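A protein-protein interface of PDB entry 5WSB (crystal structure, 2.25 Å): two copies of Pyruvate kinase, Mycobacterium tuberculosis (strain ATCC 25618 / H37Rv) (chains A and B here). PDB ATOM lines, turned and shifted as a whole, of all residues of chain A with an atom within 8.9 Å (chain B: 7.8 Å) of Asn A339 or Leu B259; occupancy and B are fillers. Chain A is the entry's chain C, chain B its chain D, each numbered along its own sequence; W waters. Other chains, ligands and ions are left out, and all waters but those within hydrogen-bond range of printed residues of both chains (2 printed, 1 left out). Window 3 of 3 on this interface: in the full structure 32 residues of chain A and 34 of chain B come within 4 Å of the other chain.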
ATOM      1  N   ALA A 296      30.414   7.291 -25.369  1.00  0.00           N
ATOM      2  CA  ALA A 296      29.208   7.348 -26.179  1.00  0.00           C
ATOM      3  C   ALA A 296      28.016   7.833 -25.329  1.00  0.00           C
ATOM      4  O   ALA A 296      27.152   8.589 -25.794  1.00  0.00           O
ATOM      5  CB  ALA A 296      28.923   5.992 -26.781  1.00  0.00           C
ATOM      6  N   SER A 297      27.972   7.398 -24.089  1.00  0.00           N
ATOM      7  CA  SER A 297      26.975   7.891 -23.133  1.00  0.00           C
ATOM      8  C   SER A 297      27.121   9.409 -22.907  1.00  0.00           C
ATOM      9  O   SER A 297      26.132  10.146 -22.823  1.00  0.00           O
ATOM     10  CB  SER A 297      27.141   7.124 -21.780  1.00  0.00           C
ATOM     11  OG  SER A 297      26.290   7.634 -20.747  1.00  0.00           O
ATOM     12  N   ALA A 300      25.657  11.345 -25.902  1.00  0.00           N
ATOM     13  CA  ALA A 300      24.189  11.262 -25.901  1.00  0.00           C
ATOM     14  C   ALA A 300      23.550  12.125 -24.814  1.00  0.00           C
ATOM     15  O   ALA A 300      22.479  12.699 -25.002  1.00  0.00           O
ATOM     16  CB  ALA A 300      23.743   9.823 -25.689  1.00  0.00           C
ATOM     17  N   ASN A 301      24.172  12.148 -23.650  1.00  0.00           N
ATOM     18  CA  ASN A 301      23.571  12.804 -22.518  1.00  0.00           C
ATOM     19  C   ASN A 301      23.812  14.302 -22.599  1.00  0.00           C
ATOM     20  O   ASN A 301      23.061  15.085 -22.034  1.00  0.00           O
ATOM     21  CB  ASN A 301      24.113  12.210 -21.195  1.00  0.00           C
ATOM     22  CG  ASN A 301      23.302  10.998 -20.719  1.00  0.00           C
ATOM     23  OD1 ASN A 301      22.093  11.104 -20.443  1.00  0.00           O
ATOM     24  ND2 ASN A 301      23.970   9.837 -20.608  1.00  0.00           N
ATOM     25  N   VAL A 303      23.536  15.768 -25.481  1.00  0.00           N
ATOM     26  CA  VAL A 303      22.425  16.125 -26.355  1.00  0.00           C
ATOM     27  C   VAL A 303      21.139  16.279 -25.555  1.00  0.00           C
ATOM     28  O   VAL A 303      20.396  17.258 -25.744  1.00  0.00           O
ATOM     29  CB  VAL A 303      22.200  15.066 -27.474  1.00  0.00           C
ATOM     30  CG1 VAL A 303      21.044  15.486 -28.371  1.00  0.00           C
ATOM     31  CG2 VAL A 303      23.444  14.893 -28.324  1.00  0.00           C
ATOM     32  N   LEU A 304      20.876  15.316 -24.648  1.00  0.00           N
ATOM     33  CA  LEU A 304      19.646  15.299 -23.873  1.00  0.00           C
ATOM     34  C   LEU A 304      19.602  16.444 -22.906  1.00  0.00           C
ATOM     35  O   LEU A 304      18.530  16.922 -22.586  1.00  0.00           O
ATOM     36  CB  LEU A 304      19.486  13.956 -23.130  1.00  0.00           C
ATOM     37  CG  LEU A 304      19.192  12.769 -24.066  1.00  0.00           C
ATOM     38  CD1 LEU A 304      19.417  11.418 -23.391  1.00  0.00           C
ATOM     39  CD2 LEU A 304      17.744  12.864 -24.575  1.00  0.00           C
ATOM     40  N   ILE A 332      26.310   9.403 -33.042  1.00  0.00           N
ATOM     41  CA  ILE A 332      25.709   9.342 -31.706  1.00  0.00           C
ATOM     42  C   ILE A 332      24.631  10.408 -31.504  1.00  0.00           C
ATOM     43  O   ILE A 332      23.554  10.137 -30.948  1.00  0.00           O
ATOM     44  CB  ILE A 332      26.750   9.504 -30.593  1.00  0.00           C
ATOM     45  CG1 ILE A 332      27.776   8.367 -30.632  1.00  0.00           C
ATOM     46  CG2 ILE A 332      26.058   9.449 -29.241  1.00  0.00           C
ATOM     47  CD1 ILE A 332      29.056   8.658 -29.861  1.00  0.00           C
ATOM     48  N   ILE A 333      24.939  11.629 -31.930  1.00  0.00           N
ATOM     49  CA  ILE A 333      24.003  12.722 -31.815  1.00  0.00           C
ATOM     50  C   ILE A 333      22.758  12.404 -32.619  1.00  0.00           C
ATOM     51  O   ILE A 333      21.635  12.691 -32.200  1.00  0.00           O
ATOM     52  CB  ILE A 333      24.609  14.058 -32.310  1.00  0.00           C
ATOM     53  CG1 ILE A 333      25.734  14.518 -31.383  1.00  0.00           C
ATOM     54  CG2 ILE A 333      23.547  15.148 -32.334  1.00  0.00           C
ATOM     55  CD1 ILE A 333      26.569  15.656 -31.958  1.00  0.00           C
ATOM     56  N   CYS A 334      22.952  11.780 -33.770  1.00  0.00           N
ATOM     57  CA  CYS A 334      21.832  11.516 -34.677  1.00  0.00           C
ATOM     58  C   CYS A 334      20.957  10.396 -34.140  1.00  0.00           C
ATOM     59  O   CYS A 334      19.727  10.432 -34.286  1.00  0.00           O
ATOM     60  CB  CYS A 334      22.325  11.201 -36.095  1.00  0.00           C
ATOM     61  SG  CYS A 334      22.865  12.671 -37.008  1.00  0.00           S
ATOM     62  N   ALA A 335      21.580   9.396 -33.534  1.00  0.00           N
ATOM     63  CA  ALA A 335      20.827   8.318 -32.964  1.00  0.00           C
ATOM     64  C   ALA A 335      19.887   8.905 -31.913  1.00  0.00           C
ATOM     65  O   ALA A 335      18.701   8.571 -31.879  1.00  0.00           O
ATOM     66  CB  ALA A 335      21.752   7.293 -32.357  1.00  0.00           C
ATOM     67  N   VAL A 336      20.389   9.840 -31.102  1.00  0.00           N
ATOM     68  CA  VAL A 336      19.572  10.407 -30.017  1.00  0.00           C
ATOM     69  C   VAL A 336      18.423  11.280 -30.546  1.00  0.00           C
ATOM     70  O   VAL A 336      17.273  11.202 -30.048  1.00  0.00           O
ATOM     71  CB  VAL A 336      20.447  11.202 -29.030  1.00  0.00           C
ATOM     72  CG1 VAL A 336      19.605  11.955 -28.020  1.00  0.00           C
ATOM     73  CG2 VAL A 336      21.405  10.267 -28.328  1.00  0.00           C
ATOM     74  N   GLU A 337      18.715  12.072 -31.592  1.00  0.00           N
ATOM     75  CA  GLU A 337      17.757  13.035 -32.142  1.00  0.00           C
ATOM     76  C   GLU A 337      16.649  12.351 -32.914  1.00  0.00           C
ATOM     77  O   GLU A 337      15.477  12.804 -32.899  1.00  0.00           O
ATOM     78  CB  GLU A 337      18.480  14.065 -33.006  1.00  0.00           C
ATOM     79  CG  GLU A 337      19.339  15.056 -32.219  1.00  0.00           C
ATOM     80  CD  GLU A 337      20.252  15.892 -33.139  1.00  0.00           C
ATOM     81  OE1 GLU A 337      20.258  15.661 -34.371  1.00  0.00           O
ATOM     82  OE2 GLU A 337      20.981  16.769 -32.623  1.00  0.00           O
ATOM     83  N   GLU A 338      17.002  11.270 -33.600  1.00  0.00           N
ATOM     84  CA  GLU A 338      16.004  10.462 -34.296  1.00  0.00           C
ATOM     85  C   GLU A 338      14.954   9.982 -33.296  1.00  0.00           C
ATOM     86  O   GLU A 338      13.769   9.933 -33.597  1.00  0.00           O
ATOM     87  CB  GLU A 338      16.651   9.264 -34.984  1.00  0.00           C
ATOM     88  CG  GLU A 338      15.901   8.803 -36.228  1.00  0.00           C
ATOM     89  CD  GLU A 338      16.164   7.338 -36.574  1.00  0.00           C
ATOM     90  OE1 GLU A 338      16.577   6.574 -35.660  1.00  0.00           O
ATOM     91  OE2 GLU A 338      15.942   6.958 -37.754  1.00  0.00           O
ATOM     92  N   ASN A 339      15.383   9.613 -32.101  1.00  0.00           N
ATOM     93  CA  ASN A 339      14.414   9.299 -31.062  1.00  0.00           C
ATOM     94  C   ASN A 339      13.611  10.554 -30.682  1.00  0.00           C
ATOM     95  O   ASN A 339      12.394  10.542 -30.710  1.00  0.00           O
ATOM     96  CB  ASN A 339      15.090   8.721 -29.839  1.00  0.00           C
ATOM     97  CG  ASN A 339      14.096   8.305 -28.797  1.00  0.00           C
ATOM     98  OD1 ASN A 339      13.935   8.983 -27.778  1.00  0.00           O
ATOM     99  ND2 ASN A 339      13.374   7.214 -29.064  1.00  0.00           N
ATOM    100  N   SER A 340      14.296  11.636 -30.339  1.00  0.00           N
ATOM    101  CA  SER A 340      13.616  12.866 -29.945  1.00  0.00           C
ATOM    102  C   SER A 340      14.569  14.034 -29.808  1.00  0.00           C
ATOM    103  O   SER A 340      15.684  13.884 -29.327  1.00  0.00           O
ATOM    104  CB  SER A 340      12.889  12.670 -28.609  1.00  0.00           C
ATOM    105  OG  SER A 340      12.263  13.864 -28.200  1.00  0.00           O
ATOM    106  N   THR A 341      14.089  15.208 -30.203  1.00  0.00           N
ATOM    107  CA  THR A 341      14.841  16.437 -30.148  1.00  0.00           C
ATOM    108  C   THR A 341      14.508  17.196 -28.875  1.00  0.00           C
ATOM    109  O   THR A 341      14.998  18.324 -28.661  1.00  0.00           O
ATOM    110  CB  THR A 341      14.503  17.352 -31.353  1.00  0.00           C
ATOM    111  OG1 THR A 341      13.093  17.597 -31.388  1.00  0.00           O
ATOM    112  CG2 THR A 341      14.906  16.693 -32.655  1.00  0.00           C
ATOM    113  N   ALA A 342      13.685  16.586 -28.020  1.00  0.00           N
ATOM    114  CA  ALA A 342      13.323  17.160 -26.737  1.00  0.00           C
ATOM    115  C   ALA A 342      14.534  17.634 -25.979  1.00  0.00           C
ATOM    116  O   ALA A 342      15.591  17.012 -26.005  1.00  0.00           O
ATOM    117  CB  ALA A 342      12.541  16.163 -25.896  1.00  0.00           C
ATOM    118  N   PRO A 392      11.527  19.302 -33.919  1.00  0.00           N
ATOM    119  CA  PRO A 392      11.957  18.438 -34.996  1.00  0.00           C
ATOM    120  C   PRO A 392      11.934  19.094 -36.384  1.00  0.00           C
ATOM    121  O   PRO A 392      12.422  18.500 -37.327  1.00  0.00           O
ATOM    122  CB  PRO A 392      10.969  17.259 -34.933  1.00  0.00           C
ATOM    123  CG  PRO A 392       9.748  17.825 -34.322  1.00  0.00           C
ATOM    124  CD  PRO A 392      10.227  18.889 -33.367  1.00  0.00           C
ATOM    125  N   ILE B 228      16.822  -7.194 -26.408  1.00  0.00           N
ATOM    126  CA  ILE B 228      16.196  -5.883 -26.387  1.00  0.00           C
ATOM    127  C   ILE B 228      14.841  -5.961 -27.089  1.00  0.00           C
ATOM    128  O   ILE B 228      13.882  -5.281 -26.692  1.00  0.00           O
ATOM    129  CB  ILE B 228      17.073  -4.803 -27.066  1.00  0.00           C
ATOM    130  CG1 ILE B 228      18.519  -4.825 -26.553  1.00  0.00           C
ATOM    131  CG2 ILE B 228      16.483  -3.426 -26.844  1.00  0.00           C
ATOM    132  CD1 ILE B 228      18.645  -4.714 -25.058  1.00  0.00           C
ATOM    133  N   LEU B 231      12.420  -7.198 -24.406  1.00  0.00           N
ATOM    134  CA  LEU B 231      12.860  -6.671 -23.128  1.00  0.00           C
ATOM    135  C   LEU B 231      11.841  -6.865 -22.045  1.00  0.00           C
ATOM    136  O   LEU B 231      12.189  -7.243 -20.925  1.00  0.00           O
ATOM    137  CB  LEU B 231      13.149  -5.181 -23.242  1.00  0.00           C
ATOM    138  CG  LEU B 231      13.798  -4.531 -22.020  1.00  0.00           C
ATOM    139  CD1 LEU B 231      15.192  -5.108 -21.829  1.00  0.00           C
ATOM    140  CD2 LEU B 231      13.867  -3.030 -22.226  1.00  0.00           C
ATOM    141  N   LEU B 248      27.010  -5.454 -25.854  1.00  0.00           N
ATOM    142  CA  LEU B 248      25.813  -4.848 -26.418  1.00  0.00           C
ATOM    143  C   LEU B 248      26.240  -3.807 -27.454  1.00  0.00           C
ATOM    144  O   LEU B 248      25.619  -3.661 -28.498  1.00  0.00           O
ATOM    145  CB  LEU B 248      24.956  -4.206 -25.311  1.00  0.00           C
ATOM    146  CG  LEU B 248      23.596  -3.638 -25.787  1.00  0.00           C
ATOM    147  CD1 LEU B 248      22.630  -4.712 -26.234  1.00  0.00           C
ATOM    148  CD2 LEU B 248      22.948  -2.766 -24.727  1.00  0.00           C
ATOM    149  N   LEU B 254      27.072   0.965 -31.444  1.00  0.00           N
ATOM    150  CA  LEU B 254      27.362   1.557 -30.173  1.00  0.00           C
ATOM    151  C   LEU B 254      26.604   2.843 -29.903  1.00  0.00           C
ATOM    152  O   LEU B 254      26.360   3.195 -28.743  1.00  0.00           O
ATOM    153  CB  LEU B 254      28.869   1.747 -29.983  1.00  0.00           C
ATOM    154  CG  LEU B 254      29.667   2.682 -30.877  1.00  0.00           C
ATOM    155  CD1 LEU B 254      29.512   4.139 -30.448  1.00  0.00           C
ATOM    156  CD2 LEU B 254      31.122   2.270 -30.771  1.00  0.00           C
ATOM    157  N   GLU B 255      26.202   3.538 -30.955  1.00  0.00           N
ATOM    158  CA  GLU B 255      25.442   4.771 -30.799  1.00  0.00           C
ATOM    159  C   GLU B 255      24.003   4.521 -30.259  1.00  0.00           C
ATOM    160  O   GLU B 255      23.335   5.455 -29.799  1.00  0.00           O
ATOM    161  CB  GLU B 255      25.415   5.581 -32.132  1.00  0.00           C
ATOM    162  CG  GLU B 255      24.692   4.932 -33.303  1.00  0.00           C
ATOM    163  CD  GLU B 255      25.652   4.332 -34.331  1.00  0.00           C
ATOM    164  OE1 GLU B 255      26.755   3.945 -33.903  1.00  0.00           O
ATOM    165  OE2 GLU B 255      25.290   4.241 -35.557  1.00  0.00           O
ATOM    166  N   GLU B 256      23.528   3.274 -30.324  1.00  0.00           N
ATOM    167  CA  GLU B 256      22.171   2.979 -29.899  1.00  0.00           C
ATOM    168  C   GLU B 256      22.130   2.524 -28.437  1.00  0.00           C
ATOM    169  O   GLU B 256      21.057   2.388 -27.859  1.00  0.00           O
ATOM    170  CB  GLU B 256      21.550   1.910 -30.812  1.00  0.00           C
ATOM    171  CG  GLU B 256      21.083   2.467 -32.151  1.00  0.00           C
ATOM    172  CD  GLU B 256      20.980   1.418 -33.237  1.00  0.00           C
ATOM    173  OE1 GLU B 256      20.801   0.231 -32.877  1.00  0.00           O
ATOM    174  OE2 GLU B 256      21.081   1.777 -34.446  1.00  0.00           O
ATOM    175  N   VAL B 257      23.292   2.313 -27.837  1.00  0.00           N
ATOM    176  CA  VAL B 257      23.360   1.758 -26.484  1.00  0.00           C
ATOM    177  C   VAL B 257      22.778   2.697 -25.422  1.00  0.00           C
ATOM    178  O   VAL B 257      22.086   2.258 -24.512  1.00  0.00           O
ATOM    179  CB  VAL B 257      24.794   1.378 -26.092  1.00  0.00           C
ATOM    180  CG1 VAL B 257      24.858   1.021 -24.606  1.00  0.00           C
ATOM    181  CG2 VAL B 257      25.292   0.197 -26.935  1.00  0.00           C
ATOM    182  N   PRO B 258      23.054   4.003 -25.526  1.00  0.00           N
ATOM    183  CA  PRO B 258      22.631   4.885 -24.446  1.00  0.00           C
ATOM    184  C   PRO B 258      21.145   4.949 -24.243  1.00  0.00           C
ATOM    185  O   PRO B 258      20.672   4.943 -23.112  1.00  0.00           O
ATOM    186  CB  PRO B 258      23.182   6.215 -24.869  1.00  0.00           C
ATOM    187  CG  PRO B 258      24.448   5.823 -25.536  1.00  0.00           C
ATOM    188  CD  PRO B 258      24.035   4.664 -26.383  1.00  0.00           C
ATOM    189  N   LEU B 259      20.402   4.943 -25.324  1.00  0.00           N
ATOM    190  CA  LEU B 259      18.969   4.917 -25.221  1.00  0.00           C
ATOM    191  C   LEU B 259      18.414   3.508 -24.851  1.00  0.00           C
ATOM    192  O   LEU B 259      17.343   3.387 -24.221  1.00  0.00           O
ATOM    193  CB  LEU B 259      18.321   5.448 -26.477  1.00  0.00           C
ATOM    194  CG  LEU B 259      18.393   6.972 -26.620  1.00  0.00           C
ATOM    195  CD1 LEU B 259      17.950   7.408 -28.011  1.00  0.00           C
ATOM    196  CD2 LEU B 259      17.554   7.685 -25.598  1.00  0.00           C
ATOM    197  N   VAL B 260      19.109   2.452 -25.238  1.00  0.00           N
ATOM    198  CA  VAL B 260      18.665   1.132 -24.815  1.00  0.00           C
ATOM    199  C   VAL B 260      18.810   1.033 -23.288  1.00  0.00           C
ATOM    200  O   VAL B 260      17.872   0.695 -22.587  1.00  0.00           O
ATOM    201  CB  VAL B 260      19.452   0.024 -25.511  1.00  0.00           C
ATOM    202  CG1 VAL B 260      19.154  -1.314 -24.857  1.00  0.00           C
ATOM    203  CG2 VAL B 260      19.111   0.011 -26.998  1.00  0.00           C
ATOM    204  N   GLN B 261      19.990   1.381 -22.791  1.00  0.00           N
ATOM    205  CA  GLN B 261      20.240   1.498 -21.376  1.00  0.00           C
ATOM    206  C   GLN B 261      19.090   2.164 -20.632  1.00  0.00           C
ATOM    207  O   GLN B 261      18.569   1.613 -19.620  1.00  0.00           O
ATOM    208  CB  GLN B 261      21.549   2.262 -21.102  1.00  0.00           C
ATOM    209  CG  GLN B 261      21.835   2.491 -19.606  1.00  0.00           C
ATOM    210  CD  GLN B 261      23.123   3.210 -19.336  1.00  0.00           C
ATOM    211  OE1 GLN B 261      24.183   2.804 -19.842  1.00  0.00           O
ATOM    212  NE2 GLN B 261      23.069   4.250 -18.494  1.00  0.00           N
ATOM    213  N   LYS B 262      18.700   3.347 -21.067  1.00  0.00           N
ATOM    214  CA  LYS B 262      17.704   4.124 -20.317  1.00  0.00           C
ATOM    215  C   LYS B 262      16.333   3.462 -20.341  1.00  0.00           C
ATOM    216  O   LYS B 262      15.607   3.455 -19.316  1.00  0.00           O
ATOM    217  CB  LYS B 262      17.624   5.549 -20.836  1.00  0.00           C
ATOM    218  CG  LYS B 262      18.924   6.335 -20.613  1.00  0.00           C
ATOM    219  CD  LYS B 262      19.096   7.474 -21.637  1.00  0.00           C
ATOM    220  CE  LYS B 262      20.320   8.323 -21.322  1.00  0.00           C
ATOM    221  NZ  LYS B 262      20.083   9.165 -20.122  1.00  0.00           N
ATOM    222  N   ARG B 263      15.973   2.890 -21.485  1.00  0.00           N
ATOM    223  CA  ARG B 263      14.713   2.161 -21.593  1.00  0.00           C
ATOM    224  C   ARG B 263      14.729   0.860 -20.740  1.00  0.00           C
ATOM    225  O   ARG B 263      13.696   0.417 -20.254  1.00  0.00           O
ATOM    226  CB  ARG B 263      14.425   1.830 -23.059  1.00  0.00           C
ATOM    227  CG  ARG B 263      14.468   3.027 -24.031  1.00  0.00           C
ATOM    228  CD  ARG B 263      14.530   2.539 -25.459  1.00  0.00           C
ATOM    229  NE  ARG B 263      13.615   1.433 -25.583  1.00  0.00           N
ATOM    230  CZ  ARG B 263      13.802   0.333 -26.295  1.00  0.00           C
ATOM    231  NH1 ARG B 263      14.906   0.154 -27.032  1.00  0.00           N
ATOM    232  NH2 ARG B 263      12.845  -0.606 -26.264  1.00  0.00           N
ATOM    233  N   ALA B 264      15.906   0.276 -20.554  1.00  0.00           N
ATOM    234  CA  ALA B 264      16.007  -0.980 -19.860  1.00  0.00           C
ATOM    235  C   ALA B 264      15.868  -0.745 -18.382  1.00  0.00           C
ATOM    236  O   ALA B 264      15.225  -1.504 -17.710  1.00  0.00           O
ATOM    237  CB  ALA B 264      17.329  -1.662 -20.171  1.00  0.00           C
ATOM    238  N   ILE B 265      16.483   0.324 -17.885  1.00  0.00           N
ATOM    239  CA  ILE B 265      16.333   0.742 -16.503  1.00  0.00           C
ATOM    240  C   ILE B 265      14.875   1.090 -16.150  1.00  0.00           C
ATOM    241  O   ILE B 265      14.371   0.702 -15.100  1.00  0.00           O
ATOM    242  CB  ILE B 265      17.262   1.958 -16.189  1.00  0.00           C
ATOM    243  CG1 ILE B 265      18.738   1.544 -16.290  1.00  0.00           C
ATOM    244  CG2 ILE B 265      17.005   2.497 -14.784  1.00  0.00           C
ATOM    245  CD1 ILE B 265      19.717   2.708 -16.247  1.00  0.00           C
ATOM    246  N   ASP B 305      19.379   8.145 -14.329  1.00  0.00           N
ATOM    247  CA  ASP B 305      18.531   7.212 -15.098  1.00  0.00           C
ATOM    248  C   ASP B 305      17.679   6.372 -14.194  1.00  0.00           C
ATOM    249  O   ASP B 305      16.594   5.923 -14.573  1.00  0.00           O
ATOM    250  CB  ASP B 305      19.412   6.249 -15.926  1.00  0.00           C
ATOM    251  CG  ASP B 305      20.054   6.920 -17.148  1.00  0.00           C
ATOM    252  OD1 ASP B 305      19.605   8.015 -17.517  1.00  0.00           O
ATOM    253  OD2 ASP B 305      20.995   6.318 -17.762  1.00  0.00           O
HETATM  254  O   HOH W   1      23.593   5.944 -22.020  1.00  0.00           O
HETATM  255  O   HOH W   2      24.869   6.088 -18.517  1.00  0.00           O
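The side-chain amide oxygen (OD1) of Asn A301 is in hydrogen-bond range of the side-chain amino group (NZ) of Lys B262 (2.8 Å).
O of Ser A297 lies within hydrogen-bond range of ND2 of Asn A301 (3.1 Å). The side-chain amino group (NZ) of Lys B262 lies within salt-bridge range of the side-chain carboxylate (OD1) of Asp B305.
Among the printed residues, merely in contact across the chains: Ala A296 with Pro B258 (3.9 Å), Ala A300 with Pro B258 (3.7 Å), Leu A304 with Lys B262 (3.8 Å), Ile A332 with Glu B255 (3.8 Å), Ala A335 with Glu B255 (3.5 Å), Val A336 with Leu B259 (3.96 Å) and Asn A339 with Leu B259 (3.6 Å).
Of the printed residues of chain B, Ala A300 touches Pro B258. Of the printed residues of chain B, Val A336 touches Leu B259. Printed residues of chain B within 4 Å of Asn A339: Leu B259. Printed residues of chain A within 4 Å of Glu B255: Ile A332 (3.8 Å) and Ala A335 (3.5 Å). Of chain A, only Ala A296 (3.9 Å) and Ala A300 (3.7 Å) come within 4 Å of Pro B258. Leu B259 touches just these residues of chain A: Val A336 (3.96 Å) and Asn A339 (3.6 Å). The nearest residue of chain B that does not touch Asn A339 is Arg B263 (6.0 Å). The nearest residue of chain A that does not touch Leu B259 is Ala A335 (4.1 Å).
Of the 18 printed residues of chain A, 8 touch a printed residue of chain B. Hydrophobic or aromatic side chains of chain A that line the printed part of chain B: Ala A300, Leu A304, Ile A332 and Ala A335. Along chain A the printed residues that touch a printed residue of chain B span positions 296 to 339. Printed residues of chain B that touch a printed residue of chain A: Glu B255, Pro B258, Leu B259 and Lys B262. Among the printed residues, 8 pairs touch across the chains. Among the printed residues, no Asp or Glu carboxylate lies within 4 Å of a Lys or Arg side-chain nitrogen of the other chain.
No position is printed for both chains. Of the 8 pairs that touch across the chains among the printed residues, none has its exchanged pair printed and touching as well.
Water W2 bridges NE2 of Gln B261 (2.6 Å) and OG of Ser A297 (3.1 Å). Water W1 bridges the backbone carbonyl oxygen (O) of Pro B258 (3.3 Å) and the side-chain hydroxyl (OG) of Ser A297 (3.4 Å).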
